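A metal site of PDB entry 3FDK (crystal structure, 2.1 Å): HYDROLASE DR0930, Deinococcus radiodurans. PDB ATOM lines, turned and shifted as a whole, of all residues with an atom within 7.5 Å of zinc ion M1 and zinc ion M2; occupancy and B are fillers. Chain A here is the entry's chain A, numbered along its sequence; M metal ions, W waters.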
ATOM      1  N   HIS A  21      27.252  24.758  12.712  1.00  0.00           N
ATOM      2  CA  HIS A  21      26.026  24.703  11.929  1.00  0.00           C
ATOM      3  C   HIS A  21      26.371  24.623  10.447  1.00  0.00           C
ATOM      4  O   HIS A  21      26.662  25.633   9.824  1.00  0.00           O
ATOM      5  CB  HIS A  21      25.152  25.941  12.162  1.00  0.00           C
ATOM      6  CG  HIS A  21      23.784  25.838  11.555  1.00  0.00           C
ATOM      7  ND1 HIS A  21      22.632  26.009  12.289  1.00  0.00           N
ATOM      8  CD2 HIS A  21      23.394  25.587  10.279  1.00  0.00           C
ATOM      9  CE1 HIS A  21      21.579  25.859  11.498  1.00  0.00           C
ATOM     10  NE2 HIS A  21      22.015  25.605  10.275  1.00  0.00           N
ATOM     11  N   GLU A  22      26.310  23.416   9.916  1.00  0.00           N
ATOM     12  CA  GLU A  22      26.580  23.187   8.500  1.00  0.00           C
ATOM     13  C   GLU A  22      25.640  22.076   8.030  1.00  0.00           C
ATOM     14  O   GLU A  22      24.974  21.428   8.830  1.00  0.00           O
ATOM     15  CB  GLU A  22      28.028  22.743   8.299  1.00  0.00           C
ATOM     16  CG  GLU A  22      29.076  23.656   8.911  1.00  0.00           C
ATOM     17  CD  GLU A  22      29.234  24.974   8.180  1.00  0.00           C
ATOM     18  OE1 GLU A  22      28.799  25.039   7.020  1.00  0.00           O
ATOM     19  OE2 GLU A  22      29.782  25.933   8.773  1.00  0.00           O
ATOM     20  N   HIS A  23      25.616  21.853   6.720  1.00  0.00           N
ATOM     21  CA  HIS A  23      24.767  20.837   6.133  1.00  0.00           C
ATOM     22  C   HIS A  23      25.543  20.005   5.105  1.00  0.00           C
ATOM     23  O   HIS A  23      25.842  20.495   4.014  1.00  0.00           O
ATOM     24  CB  HIS A  23      23.572  21.496   5.438  1.00  0.00           C
ATOM     25  CG  HIS A  23      22.637  22.198   6.375  1.00  0.00           C
ATOM     26  ND1 HIS A  23      21.801  21.520   7.232  1.00  0.00           N
ATOM     27  CD2 HIS A  23      22.427  23.510   6.611  1.00  0.00           C
ATOM     28  CE1 HIS A  23      21.125  22.382   7.957  1.00  0.00           C
ATOM     29  NE2 HIS A  23      21.486  23.607   7.601  1.00  0.00           N
ATOM     30  N   PHE A  26      21.413  18.404   2.061  1.00  0.00           N
ATOM     31  CA  PHE A  26      20.196  19.116   2.439  1.00  0.00           C
ATOM     32  C   PHE A  26      19.227  19.118   1.270  1.00  0.00           C
ATOM     33  O   PHE A  26      19.632  19.219   0.116  1.00  0.00           O
ATOM     34  CB  PHE A  26      20.525  20.570   2.799  1.00  0.00           C
ATOM     35  CG  PHE A  26      19.342  21.340   3.326  1.00  0.00           C
ATOM     36  CD1 PHE A  26      19.073  21.400   4.693  1.00  0.00           C
ATOM     37  CD2 PHE A  26      18.483  22.001   2.452  1.00  0.00           C
ATOM     38  CE1 PHE A  26      17.975  22.093   5.175  1.00  0.00           C
ATOM     39  CE2 PHE A  26      17.371  22.704   2.927  1.00  0.00           C
ATOM     40  CZ  PHE A  26      17.121  22.748   4.295  1.00  0.00           C
ATOM     41  N   ASP A  66      26.114  18.951  12.095  1.00  0.00           N
ATOM     42  CA  ASP A  66      25.203  18.976  10.959  1.00  0.00           C
ATOM     43  C   ASP A  66      23.817  19.322  11.504  1.00  0.00           C
ATOM     44  O   ASP A  66      23.235  18.569  12.288  1.00  0.00           O
ATOM     45  CB  ASP A  66      25.167  17.613  10.283  1.00  0.00           C
ATOM     46  CG  ASP A  66      24.284  17.609   9.065  1.00  0.00           C
ATOM     47  OD1 ASP A  66      23.043  17.633   9.229  1.00  0.00           O
ATOM     48  OD2 ASP A  66      24.835  17.591   7.937  1.00  0.00           O
ATOM     49  N   ALA A  67      23.292  20.477  11.096  1.00  0.00           N
ATOM     50  CA  ALA A  67      22.012  20.979  11.580  1.00  0.00           C
ATOM     51  C   ALA A  67      20.764  20.579  10.806  1.00  0.00           C
ATOM     52  O   ALA A  67      19.670  21.089  11.062  1.00  0.00           O
ATOM     53  CB  ALA A  67      22.082  22.492  11.671  1.00  0.00           C
ATOM     54  N   THR A  68      20.915  19.656   9.867  1.00  0.00           N
ATOM     55  CA  THR A  68      19.794  19.251   9.031  1.00  0.00           C
ATOM     56  C   THR A  68      18.583  18.671   9.779  1.00  0.00           C
ATOM     57  O   THR A  68      18.697  17.645  10.436  1.00  0.00           O
ATOM     58  CB  THR A  68      20.233  18.210   7.993  1.00  0.00           C
ATOM     59  OG1 THR A  68      21.484  18.628   7.421  1.00  0.00           O
ATOM     60  CG2 THR A  68      19.189  18.096   6.907  1.00  0.00           C
ATOM     61  N   PRO A  69      17.420  19.319   9.660  1.00  0.00           N
ATOM     62  CA  PRO A  69      16.210  18.830  10.330  1.00  0.00           C
ATOM     63  C   PRO A  69      15.749  17.503   9.721  1.00  0.00           C
ATOM     64  O   PRO A  69      16.065  17.187   8.565  1.00  0.00           O
ATOM     65  CB  PRO A  69      15.189  19.945  10.069  1.00  0.00           C
ATOM     66  CG  PRO A  69      16.042  21.179   9.823  1.00  0.00           C
ATOM     67  CD  PRO A  69      17.185  20.626   9.007  1.00  0.00           C
ATOM     68  N   TYR A  97      11.900  21.409  10.738  1.00  0.00           N
ATOM     69  CA  TYR A  97      12.179  22.758  10.292  1.00  0.00           C
ATOM     70  C   TYR A  97      11.022  23.688  10.639  1.00  0.00           C
ATOM     71  O   TYR A  97       9.956  23.239  11.057  1.00  0.00           O
ATOM     72  CB  TYR A  97      12.443  22.747   8.779  1.00  0.00           C
ATOM     73  CG  TYR A  97      13.295  23.881   8.249  1.00  0.00           C
ATOM     74  CD1 TYR A  97      14.423  24.326   8.944  1.00  0.00           C
ATOM     75  CD2 TYR A  97      13.015  24.450   7.008  1.00  0.00           C
ATOM     76  CE1 TYR A  97      15.261  25.311   8.399  1.00  0.00           C
ATOM     77  CE2 TYR A  97      13.836  25.421   6.464  1.00  0.00           C
ATOM     78  CZ  TYR A  97      14.954  25.844   7.153  1.00  0.00           C
ATOM     79  OH  TYR A  97      15.758  26.813   6.593  1.00  0.00           O
ATOM     80  N   TYR A  98      11.227  24.994  10.482  1.00  0.00           N
ATOM     81  CA  TYR A  98      10.194  25.955  10.815  1.00  0.00           C
ATOM     82  C   TYR A  98       8.983  25.820   9.904  1.00  0.00           C
ATOM     83  O   TYR A  98       9.066  25.267   8.804  1.00  0.00           O
ATOM     84  CB  TYR A  98      10.759  27.383  10.821  1.00  0.00           C
ATOM     85  CG  TYR A  98      10.941  28.061   9.484  1.00  0.00           C
ATOM     86  CD1 TYR A  98      10.091  29.079   9.089  1.00  0.00           C
ATOM     87  CD2 TYR A  98      11.997  27.714   8.628  1.00  0.00           C
ATOM     88  CE1 TYR A  98      10.286  29.767   7.897  1.00  0.00           C
ATOM     89  CE2 TYR A  98      12.206  28.400   7.434  1.00  0.00           C
ATOM     90  CZ  TYR A  98      11.348  29.427   7.075  1.00  0.00           C
ATOM     91  OH  TYR A  98      11.532  30.113   5.909  1.00  0.00           O
ATOM     92  N   KCX A 143      17.555  20.298  17.026  1.00  0.00           N
ATOM     93  CA  KCX A 143      17.436  21.457  16.152  1.00  0.00           C
ATOM     94  CB  KCX A 143      17.744  21.068  14.697  1.00  0.00           C
ATOM     95  CG  KCX A 143      17.422  22.133  13.630  1.00  0.00           C
ATOM     96  CD  KCX A 143      18.290  23.392  13.747  1.00  0.00           C
ATOM     97  CE  KCX A 143      18.014  24.376  12.617  1.00  0.00           C
ATOM     98  NZ  KCX A 143      18.593  23.910  11.373  1.00  0.00           N
ATOM     99  C   KCX A 143      16.027  22.044  16.240  1.00  0.00           C
ATOM    100  O   KCX A 143      15.047  21.335  16.047  1.00  0.00           O
ATOM    101  CX  KCX A 143      18.810  24.730  10.330  1.00  0.00           C
ATOM    102  OQ1 KCX A 143      19.340  24.175   9.290  1.00  0.00           O
ATOM    103  OQ2 KCX A 143      18.530  25.989  10.356  1.00  0.00           O
ATOM    104  N   LEU A 144      15.937  23.345  16.519  1.00  0.00           N
ATOM    105  CA  LEU A 144      14.662  24.052  16.579  1.00  0.00           C
ATOM    106  C   LEU A 144      14.677  25.181  15.552  1.00  0.00           C
ATOM    107  O   LEU A 144      15.739  25.712  15.238  1.00  0.00           O
ATOM    108  CB  LEU A 144      14.444  24.640  17.985  1.00  0.00           C
ATOM    109  CG  LEU A 144      14.254  23.651  19.130  1.00  0.00           C
ATOM    110  CD1 LEU A 144      14.200  24.418  20.455  1.00  0.00           C
ATOM    111  CD2 LEU A 144      12.974  22.851  18.926  1.00  0.00           C
ATOM    112  N   ALA A 145      13.506  25.574  15.075  1.00  0.00           N
ATOM    113  CA  ALA A 145      13.411  26.643  14.090  1.00  0.00           C
ATOM    114  C   ALA A 145      12.088  27.381  14.193  1.00  0.00           C
ATOM    115  O   ALA A 145      11.044  26.773  14.395  1.00  0.00           O
ATOM    116  CB  ALA A 145      13.565  26.072  12.673  1.00  0.00           C
ATOM    117  N   THR A 175      19.442  26.456  17.099  1.00  0.00           N
ATOM    118  CA  THR A 175      18.252  26.874  16.399  1.00  0.00           C
ATOM    119  C   THR A 175      18.476  27.624  15.100  1.00  0.00           C
ATOM    120  O   THR A 175      19.583  27.989  14.741  1.00  0.00           O
ATOM    121  CB  THR A 175      17.393  27.817  17.245  1.00  0.00           C
ATOM    122  OG1 THR A 175      17.958  29.128  17.196  1.00  0.00           O
ATOM    123  CG2 THR A 175      17.332  27.348  18.692  1.00  0.00           C
ATOM    124  N   HIS A 176      17.341  27.862  14.452  1.00  0.00           N
ATOM    125  CA  HIS A 176      17.247  28.600  13.201  1.00  0.00           C
ATOM    126  C   HIS A 176      16.319  29.771  13.468  1.00  0.00           C
ATOM    127  O   HIS A 176      15.200  29.587  13.941  1.00  0.00           O
ATOM    128  CB  HIS A 176      16.613  27.702  12.120  1.00  0.00           C
ATOM    129  CG  HIS A 176      16.083  28.454  10.930  1.00  0.00           C
ATOM    130  ND1 HIS A 176      16.744  28.483   9.720  1.00  0.00           N
ATOM    131  CD2 HIS A 176      14.944  29.169  10.763  1.00  0.00           C
ATOM    132  CE1 HIS A 176      16.026  29.177   8.846  1.00  0.00           C
ATOM    133  NE2 HIS A 176      14.939  29.602   9.447  1.00  0.00           N
ATOM    134  N   THR A 177      16.780  30.980  13.177  1.00  0.00           N
ATOM    135  CA  THR A 177      15.911  32.136  13.306  1.00  0.00           C
ATOM    136  C   THR A 177      15.744  32.580  11.852  1.00  0.00           C
ATOM    137  O   THR A 177      16.700  32.596  11.076  1.00  0.00           O
ATOM    138  CB  THR A 177      16.549  33.283  14.127  1.00  0.00           C
ATOM    139  OG1 THR A 177      17.823  33.636  13.576  1.00  0.00           O
ATOM    140  CG2 THR A 177      16.712  32.869  15.581  1.00  0.00           C
ATOM    141  N   GLN A 178      14.508  32.904  11.489  1.00  0.00           N
ATOM    142  CA  GLN A 178      14.186  33.323  10.137  1.00  0.00           C
ATOM    143  C   GLN A 178      14.298  34.833   9.953  1.00  0.00           C
ATOM    144  O   GLN A 178      13.701  35.609  10.708  1.00  0.00           O
ATOM    145  CB  GLN A 178      12.772  32.872   9.782  1.00  0.00           C
ATOM    146  CG  GLN A 178      12.328  33.154   8.345  1.00  0.00           C
ATOM    147  CD  GLN A 178      13.174  32.443   7.293  1.00  0.00           C
ATOM    148  OE1 GLN A 178      13.797  31.409   7.566  1.00  0.00           O
ATOM    149  NE2 GLN A 178      13.192  32.988   6.094  1.00  0.00           N
ATOM    150  N   GLY A 203      20.709  30.283  16.603  1.00  0.00           N
ATOM    151  CA  GLY A 203      21.319  30.455  15.295  1.00  0.00           C
ATOM    152  C   GLY A 203      20.878  31.599  14.398  1.00  0.00           C
ATOM    153  O   GLY A 203      19.922  32.321  14.672  1.00  0.00           O
ATOM    154  N   HIS A 204      21.613  31.752  13.289  1.00  0.00           N
ATOM    155  CA  HIS A 204      21.358  32.770  12.286  1.00  0.00           C
ATOM    156  C   HIS A 204      21.212  34.172  12.864  1.00  0.00           C
ATOM    157  O   HIS A 204      20.519  35.018  12.295  1.00  0.00           O
ATOM    158  CB  HIS A 204      20.114  32.412  11.455  1.00  0.00           C
ATOM    159  CG  HIS A 204      20.123  31.012  10.935  1.00  0.00           C
ATOM    160  ND1 HIS A 204      21.290  30.305  10.713  1.00  0.00           N
ATOM    161  CD2 HIS A 204      19.121  30.170  10.593  1.00  0.00           C
ATOM    162  CE1 HIS A 204      20.996  29.098  10.268  1.00  0.00           C
ATOM    163  NE2 HIS A 204      19.683  28.987  10.184  1.00  0.00           N
ATOM    164  N   ASP A 227      26.194  32.099  12.043  1.00  0.00           N
ATOM    165  CA  ASP A 227      26.372  30.874  11.274  1.00  0.00           C
ATOM    166  C   ASP A 227      26.048  30.845   9.793  1.00  0.00           C
ATOM    167  O   ASP A 227      25.840  29.763   9.230  1.00  0.00           O
ATOM    168  CB  ASP A 227      25.640  29.721  11.961  1.00  0.00           C
ATOM    169  CG  ASP A 227      24.188  30.048  12.300  1.00  0.00           C
ATOM    170  OD1 ASP A 227      23.598  30.974  11.680  1.00  0.00           O
ATOM    171  OD2 ASP A 227      23.630  29.374  13.183  1.00  0.00           O
ATOM    172  N   ARG A 228      25.986  32.017   9.176  1.00  0.00           N
ATOM    173  CA  ARG A 228      25.712  32.103   7.746  1.00  0.00           C
ATOM    174  C   ARG A 228      26.746  33.017   7.119  1.00  0.00           C
ATOM    175  O   ARG A 228      26.477  33.702   6.122  1.00  0.00           O
ATOM    176  CB  ARG A 228      24.303  32.638   7.499  1.00  0.00           C
ATOM    177  CG  ARG A 228      23.228  31.603   7.770  1.00  0.00           C
ATOM    178  CD  ARG A 228      21.835  32.120   7.451  1.00  0.00           C
ATOM    179  NE  ARG A 228      20.920  31.005   7.277  1.00  0.00           N
ATOM    180  CZ  ARG A 228      19.606  31.120   7.076  1.00  0.00           C
ATOM    181  NH1 ARG A 228      19.041  32.319   7.023  1.00  0.00           N
ATOM    182  NH2 ARG A 228      18.868  30.038   6.903  1.00  0.00           N
ATOM    183  N   HIS A 263      28.913  28.616   8.627  1.00  0.00           N
ATOM    184  CA  HIS A 263      28.452  29.092   7.303  1.00  0.00           C
ATOM    185  C   HIS A 263      27.048  28.657   6.853  1.00  0.00           C
ATOM    186  O   HIS A 263      26.484  29.258   5.932  1.00  0.00           O
ATOM    187  CB  HIS A 263      29.400  28.628   6.178  1.00  0.00           C
ATOM    188  CG  HIS A 263      30.846  28.670   6.522  1.00  0.00           C
ATOM    189  ND1 HIS A 263      31.499  27.644   7.170  1.00  0.00           N
ATOM    190  CD2 HIS A 263      31.793  29.607   6.245  1.00  0.00           C
ATOM    191  CE1 HIS A 263      32.780  27.939   7.275  1.00  0.00           C
ATOM    192  NE2 HIS A 263      32.979  29.119   6.715  1.00  0.00           N
ATOM    193  N   ASP A 264      26.511  27.604   7.453  1.00  0.00           N
ATOM    194  CA  ASP A 264      25.195  27.094   7.082  1.00  0.00           C
ATOM    195  C   ASP A 264      25.322  26.645   5.614  1.00  0.00           C
ATOM    196  O   ASP A 264      24.394  26.794   4.826  1.00  0.00           O
ATOM    197  CB  ASP A 264      24.113  28.177   7.201  1.00  0.00           C
ATOM    198  CG  ASP A 264      22.689  27.606   7.211  1.00  0.00           C
ATOM    199  OD1 ASP A 264      22.508  26.393   7.399  1.00  0.00           O
ATOM    200  OD2 ASP A 264      21.746  28.399   7.033  1.00  0.00           O
ATOM    201  N   SER A 265      26.489  26.111   5.280  1.00  0.00           N
ATOM    202  CA  SER A 265      26.729  25.649   3.922  1.00  0.00           C
ATOM    203  C   SER A 265      25.999  24.338   3.645  1.00  0.00           C
ATOM    204  O   SER A 265      25.549  23.645   4.551  1.00  0.00           O
ATOM    205  CB  SER A 265      28.220  25.442   3.708  1.00  0.00           C
ATOM    206  OG  SER A 265      28.704  24.365   4.489  1.00  0.00           O
ATOM    207  N   ILE A 266      25.885  24.000   2.366  1.00  0.00           N
ATOM    208  CA  ILE A 266      25.239  22.764   1.953  1.00  0.00           C
ATOM    209  C   ILE A 266      26.247  22.160   0.984  1.00  0.00           C
ATOM    210  O   ILE A 266      26.453  22.711  -0.104  1.00  0.00           O
ATOM    211  CB  ILE A 266      23.909  23.022   1.231  1.00  0.00           C
ATOM    212  CG1 ILE A 266      22.900  23.560   2.249  1.00  0.00           C
ATOM    213  CG2 ILE A 266      23.420  21.745   0.574  1.00  0.00           C
ATOM    214  CD1 ILE A 266      21.691  24.206   1.624  1.00  0.00           C
HETATM  215 ZN    ZN M   1      20.921  25.385   8.384  1.00  0.00          ZN
HETATM  216 ZN    ZN M   2      18.490  27.532   9.331  1.00  0.00          ZN
HETATM  217  O   HOH W   1      19.873  26.775   7.874  1.00  0.00           O
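OH of Tyr 97 touches zinc ion M2, 3.9 Å away.
Arg 228 touches zinc ion M2.
Of the 25 residues printed, 5 come within 4 Å of zinc ion M2.
Zinc ion M1 is bound by water W1 (1.8 Å), NE2 of His 23 (2.0 Å), OD1 of Asp 264 (2.1 Å), OQ1 of KCX 143 (2.2 Å) and NE2 of His 21 (2.2 Å).
The backbone carbonyl oxygen of Ala 67 sits at hydrogen-bond distance from NZ of KCX 143 (3.0 Å).
A ring nitrogen (ND1) of His 23 is in hydrogen-bond range of the side-chain hydroxyl (OG1) of Thr 68, at 2.9 Å.
The backbone NH (N) of His 23 lies within hydrogen-bond range of the backbone carbonyl oxygen (O) of Ser 265 (2.8 Å).
The side-chain amide oxygen of Gln 178 is in hydrogen-bond range of a ring nitrogen (NE2) of His 176 (2.8 Å).
N of His 176 sits at hydrogen-bond distance from O of Leu 144 (2.8 Å).
The backbone carbonyl oxygen (O) of His 204 is in hydrogen-bond range of the side-chain hydroxyl (OG1) of Thr 177, 3.3 Å away.
ND1 of His 204 is in hydrogen-bond range of OD1 of Asp 227, 2.6 Å away.
The side-chain carboxylate (OD2) of Asp 264 lies within salt-bridge range of the guanidinium group (NE) of Arg 228.
Zinc ion M2 is bound by OQ2 of KCX 143, ND1 of His 176, NE2 of His 204 and water W1.
Zinc ion M2 has four donor atoms within binding distance.
Of the 25 residues printed, 4 come within 4 Å of zinc ion M1.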
